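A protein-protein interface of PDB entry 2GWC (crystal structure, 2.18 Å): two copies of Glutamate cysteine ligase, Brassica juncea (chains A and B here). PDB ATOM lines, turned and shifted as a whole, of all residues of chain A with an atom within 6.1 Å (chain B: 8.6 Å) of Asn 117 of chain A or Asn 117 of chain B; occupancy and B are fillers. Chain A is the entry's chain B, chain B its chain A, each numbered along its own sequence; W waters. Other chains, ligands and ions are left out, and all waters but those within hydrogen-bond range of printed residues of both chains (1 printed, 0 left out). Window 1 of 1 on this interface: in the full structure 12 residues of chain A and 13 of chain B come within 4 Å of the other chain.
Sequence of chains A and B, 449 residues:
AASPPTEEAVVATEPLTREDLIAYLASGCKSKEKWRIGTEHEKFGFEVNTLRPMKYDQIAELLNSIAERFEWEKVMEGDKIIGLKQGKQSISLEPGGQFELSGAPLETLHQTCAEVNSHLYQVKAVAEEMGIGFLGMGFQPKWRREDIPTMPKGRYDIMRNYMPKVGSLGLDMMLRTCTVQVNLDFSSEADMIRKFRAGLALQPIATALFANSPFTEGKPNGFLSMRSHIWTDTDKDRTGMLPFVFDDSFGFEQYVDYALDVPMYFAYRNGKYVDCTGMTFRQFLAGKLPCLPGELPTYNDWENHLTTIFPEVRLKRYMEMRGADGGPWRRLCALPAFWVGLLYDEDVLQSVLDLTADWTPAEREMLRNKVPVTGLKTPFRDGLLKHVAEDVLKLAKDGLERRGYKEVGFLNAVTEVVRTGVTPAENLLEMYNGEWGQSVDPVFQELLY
Water W1 lies within hydrogen-bond range of the side-chain hydroxyl of Tyr 121 of chain A (2.4 Å) and the backbone carbonyl oxygen of His 110 of chain B (2.8 Å).
CA of Ala 114 of chain A touches CE2 of Tyr 121 of chain B (3.7 Å). ND2 of Asn 117 of chain A touches CD1 of Tyr 121 of chain B, at 3.4 Å. CA of Ala 114 of chain B touches CE2 of Tyr 121 of chain A, 3.6 Å away. CB of Tyr 121 of chain A touches OD1 of Asn 117 of chain B (3.5 Å).
The side-chain hydroxyl (OH) of Tyr 121 of chain A sits close to the side-chain sulfur (SG) of Cys 113 of chain B, at 3.3 Å. The side-chain hydroxyl (OH) of Tyr 121 of chain B lies close to the side-chain sulfur (SG) of Cys 113 of chain A (3.2 Å). The side-chain amide oxygen (OD1) of Asn 117 of chain B lies close to the side-chain amide oxygen (OD1) of Asn 117 of chain A.
The side-chain sulfur of Cys 113 of chain B forms a disulfide with the side-chain sulfur of Cys 333 of chain B (2.1 Å).
Cys 113 of chain A touches Tyr 121 of chain B, and with the chains exchanged Tyr 121 of chain A touches Cys 113 of chain B. Ala 114 of chain A touches Tyr 121 of chain B, and with the chains exchanged Tyr 121 of chain A touches Ala 114 of chain B. Asn 117 of chain B touches its own counterpart, Asn 117 of chain A. Asn 117 of chain A touches Tyr 121 of chain B, and with the chains exchanged Tyr 121 of chain A touches Asn 117 of chain B. Of the 7 pairs that touch across the chains among the printed residues, 7 have their exchanged pair printed and touching as well.
Hydrophobic or aromatic side chains of chain A within 4 Å of the printed part of chain B: Ala 114 and Tyr 121. Of the 23 printed residues of chain B, 4 touch a printed residue of chain A. Hydrophobic or aromatic side chains of chain B that line the printed part of chain A: Ala 114 and Tyr 121. Among the printed residues, 7 pairs touch across the chains. Among the printed residues, no Asp or Glu carboxylate lies within 4 Å of a Lys or Arg side-chain nitrogen of the other chain.
Asn 117 of chain A touches just these residues of chain B: Asn 117 (3.0 Å) and Tyr 121 (3.4 Å). Of the printed residues of chain A, Asn 117 of chain B touches Asn 117 and Tyr 121. No residue of chain B comes within 4 Å of Val 116 of chain A. Of the printed residues of chain B, Ala 114 of chain A touches Tyr 121 (3.7 Å). Of the printed residues of chain B, Tyr 121 of chain A touches Cys 113, Ala 114 and Asn 117. Of the printed residues of chain A, Ala 114 of chain B touches Tyr 121 (3.6 Å). Printed residues of chain B within 4 Å of Cys 113 of chain A: Tyr 121. Of the printed residues of chain A, Cys 113 of chain B touches Tyr 121 (3.2 Å).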
ATOM      1  N   THR A 112      -9.829   1.457  10.001  1.00  0.00           N
ATOM      2  CA  THR A 112      -8.500   1.481   9.355  1.00  0.00           C
ATOM      3  C   THR A 112      -7.730   2.742   9.704  1.00  0.00           C
ATOM      4  O   THR A 112      -6.603   2.679  10.169  1.00  0.00           O
ATOM      5  CB  THR A 112      -8.612   1.398   7.813  1.00  0.00           C
ATOM      6  OG1 THR A 112      -9.187   0.129   7.471  1.00  0.00           O
ATOM      7  CG2 THR A 112      -7.234   1.526   7.158  1.00  0.00           C
ATOM      8  N   CYS A 113      -8.358   3.887   9.484  1.00  0.00           N
ATOM      9  CA  CYS A 113      -7.698   5.145   9.670  1.00  0.00           C
ATOM     10  C   CYS A 113      -7.433   5.453  11.153  1.00  0.00           C
ATOM     11  O   CYS A 113      -6.455   6.091  11.489  1.00  0.00           O
ATOM     12  CB  CYS A 113      -8.508   6.248   9.009  1.00  0.00           C
ATOM     13  SG  CYS A 113      -7.470   7.709   8.582  1.00  0.00           S
ATOM     14  N   ALA A 114      -8.301   4.986  12.035  1.00  0.00           N
ATOM     15  CA  ALA A 114      -8.075   5.117  13.459  1.00  0.00           C
ATOM     16  C   ALA A 114      -6.903   4.228  13.888  1.00  0.00           C
ATOM     17  O   ALA A 114      -6.119   4.604  14.769  1.00  0.00           O
ATOM     18  CB  ALA A 114      -9.349   4.798  14.236  1.00  0.00           C
ATOM     19  N   GLU A 115      -6.776   3.072  13.245  1.00  0.00           N
ATOM     20  CA  GLU A 115      -5.660   2.172  13.472  1.00  0.00           C
ATOM     21  C   GLU A 115      -4.360   2.846  13.096  1.00  0.00           C
ATOM     22  O   GLU A 115      -3.396   2.815  13.876  1.00  0.00           O
ATOM     23  CB  GLU A 115      -5.862   0.859  12.710  1.00  0.00           C
ATOM     24  CG  GLU A 115      -4.809  -0.145  13.020  1.00  0.00           C
ATOM     25  CD  GLU A 115      -4.981  -1.413  12.248  1.00  0.00           C
ATOM     26  OE1 GLU A 115      -4.822  -1.329  11.005  1.00  0.00           O
ATOM     27  OE2 GLU A 115      -5.238  -2.467  12.899  1.00  0.00           O
ATOM     28  N   VAL A 116      -4.336   3.458  11.913  1.00  0.00           N
ATOM     29  CA  VAL A 116      -3.185   4.234  11.438  1.00  0.00           C
ATOM     30  C   VAL A 116      -2.821   5.326  12.426  1.00  0.00           C
ATOM     31  O   VAL A 116      -1.666   5.469  12.817  1.00  0.00           O
ATOM     32  CB  VAL A 116      -3.469   4.912  10.081  1.00  0.00           C
ATOM     33  CG1 VAL A 116      -2.339   5.891   9.719  1.00  0.00           C
ATOM     34  CG2 VAL A 116      -3.598   3.904   8.994  1.00  0.00           C
ATOM     35  N   ASN A 117      -3.818   6.115  12.811  1.00  0.00           N
ATOM     36  CA  ASN A 117      -3.602   7.198  13.753  1.00  0.00           C
ATOM     37  C   ASN A 117      -3.041   6.733  15.108  1.00  0.00           C
ATOM     38  O   ASN A 117      -2.154   7.376  15.653  1.00  0.00           O
ATOM     39  CB  ASN A 117      -4.876   8.025  13.926  1.00  0.00           C
ATOM     40  CG  ASN A 117      -4.730   9.054  15.007  1.00  0.00           C
ATOM     41  OD1 ASN A 117      -4.933   8.764  16.187  1.00  0.00           O
ATOM     42  ND2 ASN A 117      -4.366  10.257  14.621  1.00  0.00           N
ATOM     43  N   SER A 118      -3.571   5.635  15.643  1.00  0.00           N
ATOM     44  CA  SER A 118      -3.096   5.096  16.898  1.00  0.00           C
ATOM     45  C   SER A 118      -1.609   4.755  16.787  1.00  0.00           C
ATOM     46  O   SER A 118      -0.827   5.102  17.679  1.00  0.00           O
ATOM     47  CB  SER A 118      -3.895   3.875  17.326  1.00  0.00           C
ATOM     48  OG  SER A 118      -3.306   3.319  18.494  1.00  0.00           O
ATOM     49  N   HIS A 119      -1.214   4.149  15.666  1.00  0.00           N
ATOM     50  CA  HIS A 119       0.192   3.778  15.445  1.00  0.00           C
ATOM     51  C   HIS A 119       1.101   5.005  15.383  1.00  0.00           C
ATOM     52  O   HIS A 119       2.165   5.019  16.010  1.00  0.00           O
ATOM     53  CB  HIS A 119       0.350   2.962  14.162  1.00  0.00           C
ATOM     54  CG  HIS A 119       1.771   2.620  13.836  1.00  0.00           C
ATOM     55  ND1 HIS A 119       2.589   1.922  14.701  1.00  0.00           N
ATOM     56  CD2 HIS A 119       2.529   2.908  12.748  1.00  0.00           C
ATOM     57  CE1 HIS A 119       3.785   1.779  14.150  1.00  0.00           C
ATOM     58  NE2 HIS A 119       3.769   2.351  12.959  1.00  0.00           N
ATOM     59  N   LEU A 120       0.686   5.994  14.586  1.00  0.00           N
ATOM     60  CA  LEU A 120       1.462   7.210  14.387  1.00  0.00           C
ATOM     61  C   LEU A 120       1.630   7.930  15.712  1.00  0.00           C
ATOM     62  O   LEU A 120       2.710   8.459  15.990  1.00  0.00           O
ATOM     63  CB  LEU A 120       0.833   8.154  13.334  1.00  0.00           C
ATOM     64  CG  LEU A 120       0.819   7.617  11.881  1.00  0.00           C
ATOM     65  CD1 LEU A 120       0.065   8.539  10.864  1.00  0.00           C
ATOM     66  CD2 LEU A 120       2.235   7.271  11.403  1.00  0.00           C
ATOM     67  N   TYR A 121       0.570   7.933  16.533  1.00  0.00           N
ATOM     68  CA  TYR A 121       0.643   8.564  17.853  1.00  0.00           C
ATOM     69  C   TYR A 121       1.685   7.843  18.718  1.00  0.00           C
ATOM     70  O   TYR A 121       2.555   8.498  19.320  1.00  0.00           O
ATOM     71  CB  TYR A 121      -0.691   8.631  18.589  1.00  0.00           C
ATOM     72  CG  TYR A 121      -0.454   9.095  20.016  1.00  0.00           C
ATOM     73  CD1 TYR A 121      -0.293  10.444  20.310  1.00  0.00           C
ATOM     74  CD2 TYR A 121      -0.317   8.197  21.045  1.00  0.00           C
ATOM     75  CE1 TYR A 121      -0.053  10.876  21.574  1.00  0.00           C
ATOM     76  CE2 TYR A 121      -0.050   8.636  22.337  1.00  0.00           C
ATOM     77  CZ  TYR A 121       0.091   9.968  22.590  1.00  0.00           C
ATOM     78  OH  TYR A 121       0.364  10.401  23.876  1.00  0.00           O
ATOM     79  N   GLN A 122       1.601   6.512  18.781  1.00  0.00           N
ATOM     80  CA  GLN A 122       2.522   5.743  19.641  1.00  0.00           C
ATOM     81  C   GLN A 122       3.985   5.916  19.221  1.00  0.00           C
ATOM     82  O   GLN A 122       4.881   6.090  20.058  1.00  0.00           O
ATOM     83  CB  GLN A 122       2.164   4.271  19.660  1.00  0.00           C
ATOM     84  CG  GLN A 122       0.814   4.006  20.238  1.00  0.00           C
ATOM     85  CD  GLN A 122       0.601   2.542  20.504  1.00  0.00           C
ATOM     86  OE1 GLN A 122       1.471   1.711  20.216  1.00  0.00           O
ATOM     87  NE2 GLN A 122      -0.545   2.211  21.104  1.00  0.00           N
ATOM     88  N   HIS B  41     -11.943  16.259  30.441  1.00  0.00           N
ATOM     89  CA  HIS B  41     -11.751  17.596  29.874  1.00  0.00           C
ATOM     90  C   HIS B  41     -12.957  17.995  29.036  1.00  0.00           C
ATOM     91  O   HIS B  41     -13.680  17.125  28.523  1.00  0.00           O
ATOM     92  CB  HIS B  41     -10.465  17.673  29.048  1.00  0.00           C
ATOM     93  CG  HIS B  41     -10.536  16.919  27.761  1.00  0.00           C
ATOM     94  ND1 HIS B  41     -10.777  17.533  26.549  1.00  0.00           N
ATOM     95  CD2 HIS B  41     -10.460  15.595  27.502  1.00  0.00           C
ATOM     96  CE1 HIS B  41     -10.808  16.622  25.598  1.00  0.00           C
ATOM     97  NE2 HIS B  41     -10.638  15.437  26.151  1.00  0.00           N
ATOM     98  N   PHE B  70     -17.245   4.554  15.473  1.00  0.00           N
ATOM     99  CA  PHE B  70     -16.270   4.165  16.459  1.00  0.00           C
ATOM    100  C   PHE B  70     -16.852   3.299  17.578  1.00  0.00           C
ATOM    101  O   PHE B  70     -16.158   2.991  18.546  1.00  0.00           O
ATOM    102  CB  PHE B  70     -15.549   5.419  16.979  1.00  0.00           C
ATOM    103  CG  PHE B  70     -14.851   6.192  15.890  1.00  0.00           C
ATOM    104  CD1 PHE B  70     -13.824   5.602  15.166  1.00  0.00           C
ATOM    105  CD2 PHE B  70     -15.248   7.471  15.548  1.00  0.00           C
ATOM    106  CE1 PHE B  70     -13.178   6.294  14.129  1.00  0.00           C
ATOM    107  CE2 PHE B  70     -14.611   8.181  14.507  1.00  0.00           C
ATOM    108  CZ  PHE B  70     -13.589   7.600  13.797  1.00  0.00           C
ATOM    109  N   GLN B  89     -15.370   4.775  29.529  1.00  0.00           N
ATOM    110  CA  GLN B  89     -15.309   6.145  29.002  1.00  0.00           C
ATOM    111  C   GLN B  89     -16.697   6.646  28.688  1.00  0.00           C
ATOM    112  O   GLN B  89     -17.561   5.858  28.295  1.00  0.00           O
ATOM    113  CB  GLN B  89     -14.534   6.189  27.703  1.00  0.00           C
ATOM    114  CG  GLN B  89     -13.069   5.943  27.829  1.00  0.00           C
ATOM    115  CD  GLN B  89     -12.364   6.197  26.500  1.00  0.00           C
ATOM    116  OE1 GLN B  89     -11.587   7.147  26.377  1.00  0.00           O
ATOM    117  NE2 GLN B  89     -12.660   5.368  25.494  1.00  0.00           N
ATOM    118  N   LEU B 101     -15.007  14.629  27.462  1.00  0.00           N
ATOM    119  CA  LEU B 101     -14.604  13.231  27.629  1.00  0.00           C
ATOM    120  C   LEU B 101     -14.288  12.998  29.105  1.00  0.00           C
ATOM    121  O   LEU B 101     -13.504  13.744  29.694  1.00  0.00           O
ATOM    122  CB  LEU B 101     -13.365  12.878  26.770  1.00  0.00           C
ATOM    123  CG  LEU B 101     -12.750  11.460  26.955  1.00  0.00           C
ATOM    124  CD1 LEU B 101     -13.578  10.417  26.289  1.00  0.00           C
ATOM    125  CD2 LEU B 101     -11.353  11.387  26.459  1.00  0.00           C
ATOM    126  N   HIS B 110       1.034   7.611  30.043  1.00  0.00           N
ATOM    127  CA  HIS B 110       1.206   7.237  28.652  1.00  0.00           C
ATOM    128  C   HIS B 110      -0.139   6.765  28.078  1.00  0.00           C
ATOM    129  O   HIS B 110      -0.481   7.086  26.958  1.00  0.00           O
ATOM    130  CB  HIS B 110       2.271   6.119  28.473  1.00  0.00           C
ATOM    131  CG  HIS B 110       3.654   6.501  28.925  1.00  0.00           C
ATOM    132  ND1 HIS B 110       4.364   7.534  28.360  1.00  0.00           N
ATOM    133  CD2 HIS B 110       4.449   5.983  29.897  1.00  0.00           C
ATOM    134  CE1 HIS B 110       5.535   7.647  28.966  1.00  0.00           C
ATOM    135  NE2 HIS B 110       5.617   6.707  29.892  1.00  0.00           N
ATOM    136  N   GLN B 111      -0.870   5.994  28.866  1.00  0.00           N
ATOM    137  CA  GLN B 111      -2.223   5.550  28.520  1.00  0.00           C
ATOM    138  C   GLN B 111      -3.206   6.745  28.510  1.00  0.00           C
ATOM    139  O   GLN B 111      -4.050   6.849  27.618  1.00  0.00           O
ATOM    140  CB  GLN B 111      -2.706   4.463  29.500  1.00  0.00           C
ATOM    141  CG  GLN B 111      -1.899   3.182  29.498  1.00  0.00           C
ATOM    142  CD  GLN B 111      -2.131   2.336  30.732  1.00  0.00           C
ATOM    143  OE1 GLN B 111      -2.669   2.807  31.720  1.00  0.00           O
ATOM    144  NE2 GLN B 111      -1.727   1.052  30.676  1.00  0.00           N
ATOM    145  N   THR B 112      -3.083   7.635  29.499  1.00  0.00           N
ATOM    146  CA  THR B 112      -3.911   8.835  29.555  1.00  0.00           C
ATOM    147  C   THR B 112      -3.804   9.659  28.255  1.00  0.00           C
ATOM    148  O   THR B 112      -4.801  10.050  27.658  1.00  0.00           O
ATOM    149  CB  THR B 112      -3.527   9.713  30.778  1.00  0.00           C
ATOM    150  OG1 THR B 112      -3.752   8.959  31.985  1.00  0.00           O
ATOM    151  CG2 THR B 112      -4.347  11.018  30.818  1.00  0.00           C
ATOM    152  N   CYS B 113      -2.585   9.920  27.827  1.00  0.00           N
ATOM    153  CA  CYS B 113      -2.383  10.788  26.684  1.00  0.00           C
ATOM    154  C   CYS B 113      -2.782  10.136  25.365  1.00  0.00           C
ATOM    155  O   CYS B 113      -3.226  10.826  24.444  1.00  0.00           O
ATOM    156  CB  CYS B 113      -0.965  11.313  26.652  1.00  0.00           C
ATOM    157  SG  CYS B 113      -0.829  12.867  25.766  1.00  0.00           S
ATOM    158  N   ALA B 114      -2.655   8.809  25.297  1.00  0.00           N
ATOM    159  CA  ALA B 114      -3.141   8.060  24.136  1.00  0.00           C
ATOM    160  C   ALA B 114      -4.659   8.079  24.096  1.00  0.00           C
ATOM    161  O   ALA B 114      -5.254   8.129  23.020  1.00  0.00           O
ATOM    162  CB  ALA B 114      -2.610   6.642  24.122  1.00  0.00           C
ATOM    163  N   GLU B 115      -5.291   8.033  25.275  1.00  0.00           N
ATOM    164  CA  GLU B 115      -6.758   8.147  25.379  1.00  0.00           C
ATOM    165  C   GLU B 115      -7.280   9.516  24.891  1.00  0.00           C
ATOM    166  O   GLU B 115      -8.254   9.602  24.151  1.00  0.00           O
ATOM    167  CB  GLU B 115      -7.192   7.921  26.814  1.00  0.00           C
ATOM    168  CG  GLU B 115      -8.664   7.752  26.984  1.00  0.00           C
ATOM    169  CD  GLU B 115      -9.033   7.679  28.439  1.00  0.00           C
ATOM    170  OE1 GLU B 115      -8.744   8.666  29.149  1.00  0.00           O
ATOM    171  OE2 GLU B 115      -9.613   6.657  28.865  1.00  0.00           O
ATOM    172  N   VAL B 116      -6.626  10.575  25.329  1.00  0.00           N
ATOM    173  CA  VAL B 116      -6.873  11.927  24.822  1.00  0.00           C
ATOM    174  C   VAL B 116      -6.702  11.996  23.305  1.00  0.00           C
ATOM    175  O   VAL B 116      -7.582  12.485  22.603  1.00  0.00           O
ATOM    176  CB  VAL B 116      -5.910  12.959  25.508  1.00  0.00           C
ATOM    177  CG1 VAL B 116      -5.968  14.372  24.813  1.00  0.00           C
ATOM    178  CG2 VAL B 116      -6.225  13.071  27.004  1.00  0.00           C
ATOM    179  N   ASN B 117      -5.583  11.498  22.788  1.00  0.00           N
ATOM    180  CA  ASN B 117      -5.346  11.488  21.352  1.00  0.00           C
ATOM    181  C   ASN B 117      -6.415  10.695  20.590  1.00  0.00           C
ATOM    182  O   ASN B 117      -6.909  11.149  19.568  1.00  0.00           O
ATOM    183  CB  ASN B 117      -3.946  10.957  21.011  1.00  0.00           C
ATOM    184  CG  ASN B 117      -3.746  10.742  19.481  1.00  0.00           C
ATOM    185  OD1 ASN B 117      -4.042   9.669  18.946  1.00  0.00           O
ATOM    186  ND2 ASN B 117      -3.306  11.782  18.793  1.00  0.00           N
ATOM    187  N   SER B 118      -6.791   9.516  21.090  1.00  0.00           N
ATOM    188  CA  SER B 118      -7.822   8.735  20.429  1.00  0.00           C
ATOM    189  C   SER B 118      -9.144   9.527  20.300  1.00  0.00           C
ATOM    190  O   SER B 118      -9.812   9.512  19.256  1.00  0.00           O
ATOM    191  CB  SER B 118      -8.038   7.438  21.189  1.00  0.00           C
ATOM    192  OG  SER B 118      -9.176   6.767  20.716  1.00  0.00           O
ATOM    193  N   HIS B 119      -9.502  10.222  21.365  1.00  0.00           N
ATOM    194  CA  HIS B 119     -10.722  11.013  21.398  1.00  0.00           C
ATOM    195  C   HIS B 119     -10.686  12.168  20.393  1.00  0.00           C
ATOM    196  O   HIS B 119     -11.630  12.374  19.646  1.00  0.00           O
ATOM    197  CB  HIS B 119     -10.951  11.551  22.825  1.00  0.00           C
ATOM    198  CG  HIS B 119     -12.146  12.438  22.931  1.00  0.00           C
ATOM    199  ND1 HIS B 119     -13.414  12.000  22.636  1.00  0.00           N
ATOM    200  CD2 HIS B 119     -12.265  13.744  23.245  1.00  0.00           C
ATOM    201  CE1 HIS B 119     -14.270  12.992  22.797  1.00  0.00           C
ATOM    202  NE2 HIS B 119     -13.599  14.061  23.169  1.00  0.00           N
ATOM    203  N   LEU B 120      -9.591  12.915  20.408  1.00  0.00           N
ATOM    204  CA  LEU B 120      -9.391  14.051  19.522  1.00  0.00           C
ATOM    205  C   LEU B 120      -9.399  13.611  18.075  1.00  0.00           C
ATOM    206  O   LEU B 120      -9.933  14.305  17.223  1.00  0.00           O
ATOM    207  CB  LEU B 120      -8.047  14.740  19.851  1.00  0.00           C
ATOM    208  CG  LEU B 120      -7.964  15.403  21.231  1.00  0.00           C
ATOM    209  CD1 LEU B 120      -6.594  16.088  21.456  1.00  0.00           C
ATOM    210  CD2 LEU B 120      -9.086  16.409  21.445  1.00  0.00           C
ATOM    211  N   TYR B 121      -8.813  12.443  17.786  1.00  0.00           N
ATOM    212  CA  TYR B 121      -8.853  11.890  16.429  1.00  0.00           C
ATOM    213  C   TYR B 121     -10.307  11.582  16.014  1.00  0.00           C
ATOM    214  O   TYR B 121     -10.723  11.921  14.911  1.00  0.00           O
ATOM    215  CB  TYR B 121      -8.000  10.590  16.262  1.00  0.00           C
ATOM    216  CG  TYR B 121      -8.280   9.977  14.915  1.00  0.00           C
ATOM    217  CD1 TYR B 121      -7.653  10.460  13.774  1.00  0.00           C
ATOM    218  CD2 TYR B 121      -9.257   8.990  14.758  1.00  0.00           C
ATOM    219  CE1 TYR B 121      -7.953   9.956  12.525  1.00  0.00           C
ATOM    220  CE2 TYR B 121      -9.565   8.494  13.534  1.00  0.00           C
ATOM    221  CZ  TYR B 121      -8.908   8.985  12.405  1.00  0.00           C
ATOM    222  OH  TYR B 121      -9.241   8.483  11.154  1.00  0.00           O
ATOM    223  N   GLN B 122     -11.068  10.920  16.890  1.00  0.00           N
ATOM    224  CA  GLN B 122     -12.434  10.520  16.543  1.00  0.00           C
ATOM    225  C   GLN B 122     -13.360  11.728  16.304  1.00  0.00           C
ATOM    226  O   GLN B 122     -14.165  11.730  15.353  1.00  0.00           O
ATOM    227  CB  GLN B 122     -13.043   9.569  17.587  1.00  0.00           C
ATOM    228  CG  GLN B 122     -12.391   8.160  17.637  1.00  0.00           C
ATOM    229  CD  GLN B 122     -13.119   7.178  18.575  1.00  0.00           C
ATOM    230  OE1 GLN B 122     -14.131   7.513  19.194  1.00  0.00           O
ATOM    231  NE2 GLN B 122     -12.603   5.959  18.674  1.00  0.00           N
ATOM    232  N   VAL B 123     -13.238  12.721  17.168  1.00  0.00           N
ATOM    233  CA  VAL B 123     -13.995  13.956  17.099  1.00  0.00           C
ATOM    234  C   VAL B 123     -13.669  14.711  15.794  1.00  0.00           C
ATOM    235  O   VAL B 123     -14.568  15.089  15.048  1.00  0.00           O
ATOM    236  CB  VAL B 123     -13.703  14.808  18.377  1.00  0.00           C
ATOM    237  CG1 VAL B 123     -14.215  16.205  18.256  1.00  0.00           C
ATOM    238  CG2 VAL B 123     -14.329  14.140  19.590  1.00  0.00           C
ATOM    239  N   LYS B 124     -12.385  14.906  15.513  1.00  0.00           N
ATOM    240  CA  LYS B 124     -11.968  15.645  14.322  1.00  0.00           C
ATOM    241  C   LYS B 124     -12.278  14.895  13.035  1.00  0.00           C
ATOM    242  O   LYS B 124     -12.549  15.513  12.012  1.00  0.00           O
ATOM    243  CB  LYS B 124     -10.474  15.976  14.390  1.00  0.00           C
ATOM    244  CG  LYS B 124     -10.130  16.970  15.490  1.00  0.00           C
ATOM    245  CD  LYS B 124      -8.688  16.816  15.986  1.00  0.00           C
ATOM    246  CE  LYS B 124      -7.684  17.206  14.940  1.00  0.00           C
ATOM    247  NZ  LYS B 124      -6.319  17.382  15.577  1.00  0.00           N
ATOM    248  N   ALA B 125     -12.228  13.562  13.092  1.00  0.00           N
ATOM    249  CA  ALA B 125     -12.571  12.699  11.966  1.00  0.00           C
ATOM    250  C   ALA B 125     -14.010  12.896  11.488  1.00  0.00           C
ATOM    251  O   ALA B 125     -14.319  12.718  10.315  1.00  0.00           O
ATOM    252  CB  ALA B 125     -12.346  11.236  12.354  1.00  0.00           C
ATOM    253  N   TRP B 329      -3.719  20.078  23.709  1.00  0.00           N
ATOM    254  CA  TRP B 329      -3.571  18.657  24.061  1.00  0.00           C
ATOM    255  C   TRP B 329      -2.383  18.369  24.966  1.00  0.00           C
ATOM    256  O   TRP B 329      -2.480  17.539  25.837  1.00  0.00           O
ATOM    257  CB  TRP B 329      -3.548  17.739  22.797  1.00  0.00           C
ATOM    258  CG  TRP B 329      -2.244  17.698  22.001  1.00  0.00           C
ATOM    259  CD1 TRP B 329      -1.877  18.527  20.970  1.00  0.00           C
ATOM    260  CD2 TRP B 329      -1.169  16.771  22.168  1.00  0.00           C
ATOM    261  NE1 TRP B 329      -0.631  18.177  20.503  1.00  0.00           N
ATOM    262  CE2 TRP B 329      -0.181  17.097  21.218  1.00  0.00           C
ATOM    263  CE3 TRP B 329      -0.938  15.697  23.043  1.00  0.00           C
ATOM    264  CZ2 TRP B 329       1.025  16.381  21.115  1.00  0.00           C
ATOM    265  CZ3 TRP B 329       0.266  14.993  22.950  1.00  0.00           C
ATOM    266  CH2 TRP B 329       1.220  15.330  21.992  1.00  0.00           C
ATOM    267  N   LEU B 332      -3.563  19.067  28.381  1.00  0.00           N
ATOM    268  CA  LEU B 332      -4.463  18.022  28.847  1.00  0.00           C
ATOM    269  C   LEU B 332      -3.730  16.830  29.458  1.00  0.00           C
ATOM    270  O   LEU B 332      -4.274  16.169  30.328  1.00  0.00           O
ATOM    271  CB  LEU B 332      -5.361  17.530  27.718  1.00  0.00           C
ATOM    272  CG  LEU B 332      -6.309  18.588  27.149  1.00  0.00           C
ATOM    273  CD1 LEU B 332      -7.191  17.950  26.118  1.00  0.00           C
ATOM    274  CD2 LEU B 332      -7.089  19.269  28.231  1.00  0.00           C
ATOM    275  N   CYS B 333      -2.537  16.523  28.950  1.00  0.00           N
ATOM    276  CA  CYS B 333      -1.714  15.423  29.448  1.00  0.00           C
ATOM    277  C   CYS B 333      -0.857  15.883  30.635  1.00  0.00           C
ATOM    278  O   CYS B 333      -0.507  15.071  31.486  1.00  0.00           O
ATOM    279  CB  CYS B 333      -0.855  14.819  28.316  1.00  0.00           C
ATOM    280  SG  CYS B 333      -1.908  14.276  26.887  1.00  0.00           S
HETATM  281  O   HOH W   1       1.182   8.720  25.438  1.00  0.00           O
